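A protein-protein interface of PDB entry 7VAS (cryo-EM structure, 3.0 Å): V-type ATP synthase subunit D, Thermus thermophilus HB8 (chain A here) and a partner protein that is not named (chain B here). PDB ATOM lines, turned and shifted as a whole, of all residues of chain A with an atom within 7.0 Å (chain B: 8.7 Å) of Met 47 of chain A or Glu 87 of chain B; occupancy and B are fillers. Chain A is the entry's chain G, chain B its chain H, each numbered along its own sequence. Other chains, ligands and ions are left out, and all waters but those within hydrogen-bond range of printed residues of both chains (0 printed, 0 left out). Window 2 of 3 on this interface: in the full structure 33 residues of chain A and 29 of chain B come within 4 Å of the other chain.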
ATOM      1  N   LEU A  42      20.382 -15.215 -20.326  1.00  0.00           N
ATOM      2  CA  LEU A  42      19.763 -15.955 -19.234  1.00  0.00           C
ATOM      3  C   LEU A  42      20.783 -16.744 -18.421  1.00  0.00           C
ATOM      4  O   LEU A  42      20.582 -16.950 -17.221  1.00  0.00           O
ATOM      5  CB  LEU A  42      18.680 -16.885 -19.779  1.00  0.00           C
ATOM      6  CG  LEU A  42      17.247 -16.346 -19.768  1.00  0.00           C
ATOM      7  CD1 LEU A  42      16.774 -16.145 -18.339  1.00  0.00           C
ATOM      8  CD2 LEU A  42      17.133 -15.052 -20.553  1.00  0.00           C
ATOM      9  N   VAL A  43      21.871 -17.196 -19.046  1.00  0.00           N
ATOM     10  CA  VAL A  43      22.889 -17.942 -18.304  1.00  0.00           C
ATOM     11  C   VAL A  43      23.521 -17.063 -17.230  1.00  0.00           C
ATOM     12  O   VAL A  43      23.683 -17.479 -16.075  1.00  0.00           O
ATOM     13  CB  VAL A  43      23.949 -18.510 -19.265  1.00  0.00           C
ATOM     14  CG1 VAL A  43      25.135 -19.039 -18.485  1.00  0.00           C
ATOM     15  CG2 VAL A  43      23.351 -19.622 -20.099  1.00  0.00           C
ATOM     16  N   ARG A  44      23.895 -15.835 -17.595  1.00  0.00           N
ATOM     17  CA  ARG A  44      24.465 -14.918 -16.614  1.00  0.00           C
ATOM     18  C   ARG A  44      23.454 -14.580 -15.527  1.00  0.00           C
ATOM     19  O   ARG A  44      23.803 -14.516 -14.337  1.00  0.00           O
ATOM     20  CB  ARG A  44      24.956 -13.647 -17.304  1.00  0.00           C
ATOM     21  CG  ARG A  44      26.174 -13.851 -18.183  1.00  0.00           C
ATOM     22  CD  ARG A  44      26.631 -12.539 -18.795  1.00  0.00           C
ATOM     23  NE  ARG A  44      25.730 -12.083 -19.846  1.00  0.00           N
ATOM     24  CZ  ARG A  44      25.144 -10.893 -19.865  1.00  0.00           C
ATOM     25  NH1 ARG A  44      25.334 -10.014 -18.896  1.00  0.00           N
ATOM     26  NH2 ARG A  44      24.347 -10.579 -20.882  1.00  0.00           N
ATOM     27  N   GLU A  45      22.193 -14.362 -15.915  1.00  0.00           N
ATOM     28  CA  GLU A  45      21.174 -14.097 -14.902  1.00  0.00           C
ATOM     29  C   GLU A  45      21.065 -15.254 -13.911  1.00  0.00           C
ATOM     30  O   GLU A  45      20.997 -15.040 -12.691  1.00  0.00           O
ATOM     31  CB  GLU A  45      19.826 -13.828 -15.567  1.00  0.00           C
ATOM     32  CG  GLU A  45      18.699 -13.564 -14.586  1.00  0.00           C
ATOM     33  CD  GLU A  45      17.562 -12.779 -15.205  1.00  0.00           C
ATOM     34  OE1 GLU A  45      17.363 -12.885 -16.431  1.00  0.00           O
ATOM     35  OE2 GLU A  45      16.867 -12.052 -14.463  1.00  0.00           O
ATOM     36  N   ALA A  46      21.062 -16.489 -14.417  1.00  0.00           N
ATOM     37  CA  ALA A  46      20.954 -17.659 -13.552  1.00  0.00           C
ATOM     38  C   ALA A  46      22.161 -17.789 -12.635  1.00  0.00           C
ATOM     39  O   ALA A  46      22.018 -18.155 -11.464  1.00  0.00           O
ATOM     40  CB  ALA A  46      20.789 -18.923 -14.393  1.00  0.00           C
ATOM     41  N   MET A  47      23.360 -17.520 -13.154  1.00  0.00           N
ATOM     42  CA  MET A  47      24.553 -17.593 -12.315  1.00  0.00           C
ATOM     43  C   MET A  47      24.482 -16.591 -11.170  1.00  0.00           C
ATOM     44  O   MET A  47      24.790 -16.927 -10.015  1.00  0.00           O
ATOM     45  CB  MET A  47      25.804 -17.360 -13.160  1.00  0.00           C
ATOM     46  CG  MET A  47      27.084 -17.250 -12.353  1.00  0.00           C
ATOM     47  SD  MET A  47      28.539 -16.987 -13.385  1.00  0.00           S
ATOM     48  CE  MET A  47      29.593 -16.081 -12.255  1.00  0.00           C
ATOM     49  N   GLU A  48      24.068 -15.356 -11.465  1.00  0.00           N
ATOM     50  CA  GLU A  48      23.950 -14.357 -10.406  1.00  0.00           C
ATOM     51  C   GLU A  48      22.911 -14.773  -9.370  1.00  0.00           C
ATOM     52  O   GLU A  48      23.136 -14.637  -8.157  1.00  0.00           O
ATOM     53  CB  GLU A  48      23.600 -12.996 -11.007  1.00  0.00           C
ATOM     54  CG  GLU A  48      23.477 -11.881  -9.986  1.00  0.00           C
ATOM     55  CD  GLU A  48      22.046 -11.647  -9.551  1.00  0.00           C
ATOM     56  OE1 GLU A  48      21.167 -11.538 -10.431  1.00  0.00           O
ATOM     57  OE2 GLU A  48      21.801 -11.571  -8.329  1.00  0.00           O
ATOM     58  N   ALA A  49      21.767 -15.291  -9.827  1.00  0.00           N
ATOM     59  CA  ALA A  49      20.738 -15.734  -8.892  1.00  0.00           C
ATOM     60  C   ALA A  49      21.241 -16.876  -8.015  1.00  0.00           C
ATOM     61  O   ALA A  49      20.942 -16.926  -6.816  1.00  0.00           O
ATOM     62  CB  ALA A  49      19.482 -16.155  -9.652  1.00  0.00           C
ATOM     63  N   ARG A  50      22.001 -17.806  -8.598  1.00  0.00           N
ATOM     64  CA  ARG A  50      22.536 -18.917  -7.818  1.00  0.00           C
ATOM     65  C   ARG A  50      23.519 -18.430  -6.764  1.00  0.00           C
ATOM     66  O   ARG A  50      23.533 -18.937  -5.637  1.00  0.00           O
ATOM     67  CB  ARG A  50      23.202 -19.934  -8.744  1.00  0.00           C
ATOM     68  CG  ARG A  50      22.248 -20.972  -9.300  1.00  0.00           C
ATOM     69  CD  ARG A  50      22.075 -22.129  -8.338  1.00  0.00           C
ATOM     70  NE  ARG A  50      20.971 -22.997  -8.725  1.00  0.00           N
ATOM     71  CZ  ARG A  50      20.704 -24.163  -8.156  1.00  0.00           C
ATOM     72  NH1 ARG A  50      21.449 -24.638  -7.171  1.00  0.00           N
ATOM     73  NH2 ARG A  50      19.662 -24.872  -8.585  1.00  0.00           N
ATOM     74  N   LYS A  51      24.358 -17.450  -7.112  1.00  0.00           N
ATOM     75  CA  LYS A  51      25.279 -16.898  -6.121  1.00  0.00           C
ATOM     76  C   LYS A  51      24.522 -16.233  -4.975  1.00  0.00           C
ATOM     77  O   LYS A  51      24.875 -16.408  -3.797  1.00  0.00           O
ATOM     78  CB  LYS A  51      26.233 -15.905  -6.783  1.00  0.00           C
ATOM     79  CG  LYS A  51      27.147 -16.533  -7.822  1.00  0.00           C
ATOM     80  CD  LYS A  51      28.430 -15.738  -7.986  1.00  0.00           C
ATOM     81  CE  LYS A  51      28.142 -14.290  -8.335  1.00  0.00           C
ATOM     82  NZ  LYS A  51      29.397 -13.503  -8.484  1.00  0.00           N
ATOM     83  N   ALA A  52      23.476 -15.470  -5.301  1.00  0.00           N
ATOM     84  CA  ALA A  52      22.672 -14.846  -4.253  1.00  0.00           C
ATOM     85  C   ALA A  52      22.027 -15.895  -3.355  1.00  0.00           C
ATOM     86  O   ALA A  52      22.000 -15.746  -2.125  1.00  0.00           O
ATOM     87  CB  ALA A  52      21.609 -13.941  -4.873  1.00  0.00           C
ATOM     88  N   LEU A  53      21.500 -16.965  -3.954  1.00  0.00           N
ATOM     89  CA  LEU A  53      20.898 -18.032  -3.163  1.00  0.00           C
ATOM     90  C   LEU A  53      21.927 -18.695  -2.260  1.00  0.00           C
ATOM     91  O   LEU A  53      21.620 -19.047  -1.118  1.00  0.00           O
ATOM     92  CB  LEU A  53      20.248 -19.072  -4.073  1.00  0.00           C
ATOM     93  CG  LEU A  53      19.568 -20.219  -3.320  1.00  0.00           C
ATOM     94  CD1 LEU A  53      18.370 -19.705  -2.541  1.00  0.00           C
ATOM     95  CD2 LEU A  53      19.161 -21.338  -4.263  1.00  0.00           C
ATOM     96  N   THR A 143      14.202 -18.721 -12.821  1.00  0.00           N
ATOM     97  CA  THR A 143      15.232 -18.505 -13.828  1.00  0.00           C
ATOM     98  C   THR A 143      15.652 -19.821 -14.473  1.00  0.00           C
ATOM     99  O   THR A 143      15.825 -19.894 -15.696  1.00  0.00           O
ATOM    100  CB  THR A 143      16.431 -17.798 -13.206  1.00  0.00           C
ATOM    101  OG1 THR A 143      15.997 -16.566 -12.619  1.00  0.00           O
ATOM    102  CG2 THR A 143      17.454 -17.487 -14.267  1.00  0.00           C
ATOM    103  N   LEU A 147      15.635 -20.817 -18.518  1.00  0.00           N
ATOM    104  CA  LEU A 147      16.752 -21.370 -19.286  1.00  0.00           C
ATOM    105  C   LEU A 147      16.414 -22.726 -19.885  1.00  0.00           C
ATOM    106  O   LEU A 147      16.802 -23.017 -21.021  1.00  0.00           O
ATOM    107  CB  LEU A 147      18.028 -21.474 -18.448  1.00  0.00           C
ATOM    108  CG  LEU A 147      18.881 -20.232 -18.184  1.00  0.00           C
ATOM    109  CD1 LEU A 147      18.246 -19.260 -17.234  1.00  0.00           C
ATOM    110  CD2 LEU A 147      20.260 -20.657 -17.690  1.00  0.00           C
ATOM    111  N   HIS B  84      31.455 -23.993  -3.003  1.00  0.00           N
ATOM    112  CA  HIS B  84      30.456 -24.596  -3.875  1.00  0.00           C
ATOM    113  C   HIS B  84      30.823 -24.329  -5.327  1.00  0.00           C
ATOM    114  O   HIS B  84      31.046 -23.178  -5.714  1.00  0.00           O
ATOM    115  CB  HIS B  84      29.059 -24.047  -3.572  1.00  0.00           C
ATOM    116  CG  HIS B  84      27.997 -24.553  -4.497  1.00  0.00           C
ATOM    117  ND1 HIS B  84      27.714 -23.952  -5.705  1.00  0.00           N
ATOM    118  CD2 HIS B  84      27.152 -25.605  -4.393  1.00  0.00           C
ATOM    119  CE1 HIS B  84      26.739 -24.610  -6.304  1.00  0.00           C
ATOM    120  NE2 HIS B  84      26.379 -25.618  -5.529  1.00  0.00           N
ATOM    121  N   ASP B  85      30.877 -25.394  -6.126  1.00  0.00           N
ATOM    122  CA  ASP B  85      31.218 -25.287  -7.544  1.00  0.00           C
ATOM    123  C   ASP B  85      30.004 -24.754  -8.298  1.00  0.00           C
ATOM    124  O   ASP B  85      29.260 -25.484  -8.958  1.00  0.00           O
ATOM    125  CB  ASP B  85      31.674 -26.634  -8.089  1.00  0.00           C
ATOM    126  CG  ASP B  85      30.765 -27.770  -7.667  1.00  0.00           C
ATOM    127  OD1 ASP B  85      30.302 -27.762  -6.506  1.00  0.00           O
ATOM    128  OD2 ASP B  85      30.511 -28.669  -8.495  1.00  0.00           O
ATOM    129  N   VAL B  86      29.799 -23.439  -8.186  1.00  0.00           N
ATOM    130  CA  VAL B  86      28.731 -22.794  -8.942  1.00  0.00           C
ATOM    131  C   VAL B  86      29.041 -22.831 -10.435  1.00  0.00           C
ATOM    132  O   VAL B  86      28.143 -23.004 -11.266  1.00  0.00           O
ATOM    133  CB  VAL B  86      28.509 -21.358  -8.432  1.00  0.00           C
ATOM    134  CG1 VAL B  86      29.801 -20.558  -8.484  1.00  0.00           C
ATOM    135  CG2 VAL B  86      27.413 -20.668  -9.230  1.00  0.00           C
ATOM    136  N   GLU B  87      30.317 -22.682 -10.796  1.00  0.00           N
ATOM    137  CA  GLU B  87      30.706 -22.768 -12.200  1.00  0.00           C
ATOM    138  C   GLU B  87      30.510 -24.177 -12.743  1.00  0.00           C
ATOM    139  O   GLU B  87      30.096 -24.349 -13.894  1.00  0.00           O
ATOM    140  CB  GLU B  87      32.157 -22.324 -12.371  1.00  0.00           C
ATOM    141  CG  GLU B  87      32.394 -20.864 -12.032  1.00  0.00           C
ATOM    142  CD  GLU B  87      31.653 -19.928 -12.963  1.00  0.00           C
ATOM    143  OE1 GLU B  87      31.471 -20.285 -14.145  1.00  0.00           O
ATOM    144  OE2 GLU B  87      31.251 -18.836 -12.512  1.00  0.00           O
ATOM    145  N   GLY B  88      30.815 -25.196 -11.938  1.00  0.00           N
ATOM    146  CA  GLY B  88      30.619 -26.563 -12.391  1.00  0.00           C
ATOM    147  C   GLY B  88      29.159 -26.895 -12.632  1.00  0.00           C
ATOM    148  O   GLY B  88      28.814 -27.542 -13.624  1.00  0.00           O
ATOM    149  N   TYR B  89      28.283 -26.455 -11.727  1.00  0.00           N
ATOM    150  CA  TYR B  89      26.854 -26.693 -11.906  1.00  0.00           C
ATOM    151  C   TYR B  89      26.334 -26.002 -13.159  1.00  0.00           C
ATOM    152  O   TYR B  89      25.565 -26.591 -13.928  1.00  0.00           O
ATOM    153  CB  TYR B  89      26.089 -26.216 -10.672  1.00  0.00           C
ATOM    154  CG  TYR B  89      24.587 -26.271 -10.824  1.00  0.00           C
ATOM    155  CD1 TYR B  89      23.911 -27.481 -10.781  1.00  0.00           C
ATOM    156  CD2 TYR B  89      23.848 -25.113 -11.013  1.00  0.00           C
ATOM    157  CE1 TYR B  89      22.539 -27.537 -10.920  1.00  0.00           C
ATOM    158  CE2 TYR B  89      22.476 -25.159 -11.154  1.00  0.00           C
ATOM    159  CZ  TYR B  89      21.827 -26.373 -11.106  1.00  0.00           C
ATOM    160  OH  TYR B  89      20.461 -26.425 -11.246  1.00  0.00           O
ATOM    161  N   MET B  90      26.750 -24.754 -13.384  1.00  0.00           N
ATOM    162  CA  MET B  90      26.316 -24.037 -14.578  1.00  0.00           C
ATOM    163  C   MET B  90      26.854 -24.689 -15.844  1.00  0.00           C
ATOM    164  O   MET B  90      26.146 -24.769 -16.854  1.00  0.00           O
ATOM    165  CB  MET B  90      26.747 -22.574 -14.498  1.00  0.00           C
ATOM    166  CG  MET B  90      25.711 -21.677 -13.852  1.00  0.00           C
ATOM    167  SD  MET B  90      24.152 -21.693 -14.756  1.00  0.00           S
ATOM    168  CE  MET B  90      22.985 -21.779 -13.402  1.00  0.00           C
ATOM    169  N   ARG B  91      28.104 -25.153 -15.813  1.00  0.00           N
ATOM    170  CA  ARG B  91      28.665 -25.834 -16.973  1.00  0.00           C
ATOM    171  C   ARG B  91      27.904 -27.115 -17.276  1.00  0.00           C
ATOM    172  O   ARG B  91      27.608 -27.408 -18.440  1.00  0.00           O
ATOM    173  CB  ARG B  91      30.144 -26.132 -16.742  1.00  0.00           C
ATOM    174  CG  ARG B  91      31.065 -25.012 -17.173  1.00  0.00           C
ATOM    175  CD  ARG B  91      32.464 -25.195 -16.616  1.00  0.00           C
ATOM    176  NE  ARG B  91      33.068 -26.446 -17.056  1.00  0.00           N
ATOM    177  CZ  ARG B  91      34.117 -27.014 -16.477  1.00  0.00           C
ATOM    178  NH1 ARG B  91      34.701 -26.471 -15.421  1.00  0.00           N
ATOM    179  NH2 ARG B  91      34.591 -28.155 -16.969  1.00  0.00           N
ATOM    180  N   GLU B  92      27.573 -27.891 -16.242  1.00  0.00           N
ATOM    181  CA  GLU B  92      26.799 -29.109 -16.454  1.00  0.00           C
ATOM    182  C   GLU B  92      25.413 -28.792 -17.001  1.00  0.00           C
ATOM    183  O   GLU B  92      24.914 -29.487 -17.895  1.00  0.00           O
ATOM    184  CB  GLU B  92      26.696 -29.898 -15.151  1.00  0.00           C
ATOM    185  CG  GLU B  92      25.910 -31.194 -15.271  1.00  0.00           C
ATOM    186  CD  GLU B  92      25.967 -32.026 -14.007  1.00  0.00           C
ATOM    187  OE1 GLU B  92      26.071 -31.437 -12.911  1.00  0.00           O
ATOM    188  OE2 GLU B  92      25.907 -33.270 -14.108  1.00  0.00           O
ATOM    189  N   LEU B  93      24.776 -27.742 -16.478  1.00  0.00           N
ATOM    190  CA  LEU B  93      23.454 -27.358 -16.964  1.00  0.00           C
ATOM    191  C   LEU B  93      23.502 -26.930 -18.425  1.00  0.00           C
ATOM    192  O   LEU B  93      22.631 -27.305 -19.219  1.00  0.00           O
ATOM    193  CB  LEU B  93      22.886 -26.240 -16.092  1.00  0.00           C
ATOM    194  CG  LEU B  93      21.531 -25.669 -16.503  1.00  0.00           C
ATOM    195  CD1 LEU B  93      20.437 -26.705 -16.314  1.00  0.00           C
ATOM    196  CD2 LEU B  93      21.229 -24.413 -15.707  1.00  0.00           C
ATOM    197  N   VAL B  94      24.514 -26.143 -18.798  1.00  0.00           N
ATOM    198  CA  VAL B  94      24.653 -25.710 -20.185  1.00  0.00           C
ATOM    199  C   VAL B  94      24.928 -26.903 -21.089  1.00  0.00           C
ATOM    200  O   VAL B  94      24.378 -27.006 -22.192  1.00  0.00           O
ATOM    201  CB  VAL B  94      25.753 -24.639 -20.304  1.00  0.00           C
ATOM    202  CG1 VAL B  94      26.113 -24.401 -21.759  1.00  0.00           C
ATOM    203  CG2 VAL B  94      25.300 -23.344 -19.653  1.00  0.00           C
ATOM    204  N   LYS B 103      32.037 -22.550 -21.705  1.00  0.00           N
ATOM    205  CA  LYS B 103      32.354 -21.685 -20.577  1.00  0.00           C
ATOM    206  C   LYS B 103      33.631 -20.880 -20.793  1.00  0.00           C
ATOM    207  O   LYS B 103      33.903 -19.961 -20.012  1.00  0.00           O
ATOM    208  CB  LYS B 103      32.456 -22.527 -19.299  1.00  0.00           C
ATOM    209  CG  LYS B 103      32.613 -21.737 -18.003  1.00  0.00           C
ATOM    210  CD  LYS B 103      31.456 -20.771 -17.794  1.00  0.00           C
ATOM    211  CE  LYS B 103      30.155 -21.507 -17.521  1.00  0.00           C
ATOM    212  NZ  LYS B 103      29.034 -20.568 -17.248  1.00  0.00           N
ATOM    213  N   LEU B 104      34.397 -21.184 -21.838  1.00  0.00           N
ATOM    214  CA  LEU B 104      35.652 -20.490 -22.133  1.00  0.00           C
ATOM    215  C   LEU B 104      36.652 -20.651 -20.996  1.00  0.00           C
ATOM    216  O   LEU B 104      37.827 -20.937 -21.229  1.00  0.00           O
ATOM    217  CB  LEU B 104      35.400 -19.003 -22.410  1.00  0.00           C
ATOM    218  CG  LEU B 104      36.601 -18.062 -22.287  1.00  0.00           C
ATOM    219  CD1 LEU B 104      37.643 -18.352 -23.358  1.00  0.00           C
ATOM    220  CD2 LEU B 104      36.151 -16.610 -22.341  1.00  0.00           C
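The guanidinium group (NH2) of Arg 50 of chain A sits at hydrogen-bond distance from the side-chain hydroxyl (OH) of Tyr 89 of chain B (3.2 Å).
SD of Met 47 of chain A sits close to OE2 of Glu 87 of chain B, at 3.4 Å.
The side-chain carboxylate of Glu 87 of chain B is in salt-bridge range of the side-chain amino group of Lys 103 of chain B.
Ala 46 of chain A touches Met 90 of chain B.
Met 47 of chain A touches one residue of chain B.
Ala 46 of chain A touches one residue of chain B.
Of the printed residues of chain A, Met 90 of chain B touches Ala 46 (3.7 Å).
Of the printed residues of chain B, Arg 50 of chain A touches Tyr 89 (3.2 Å).
Of the printed residues of chain A, Tyr 89 of chain B touches Arg 50 (3.2 Å).
Gly 88 of chain B touches none of the printed residues of chain A.
The nearest residue of chain A that does not touch Glu 87 of chain B is Lys 51 of chain A (6.2 Å).
The nearest printed residue of chain A that does not touch Tyr 89 of chain B is Ala 46 of chain A (7.0 Å).
Of the 13 printed residues of chain B, 3 touch a printed residue of chain A.
Hydrophobic or aromatic side chains of chain B within 4 Å of the printed part of chain A: Tyr 89 and Met 90.
Printed residues of chain A that touch a printed residue of chain B: Ala 46, Met 47 and Arg 50.
Among the printed residues, 3 pairs touch across the chains.
Among the printed residues, no Asp or Glu carboxylate lies within 4 Å of a Lys or Arg side-chain nitrogen of the other chain.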
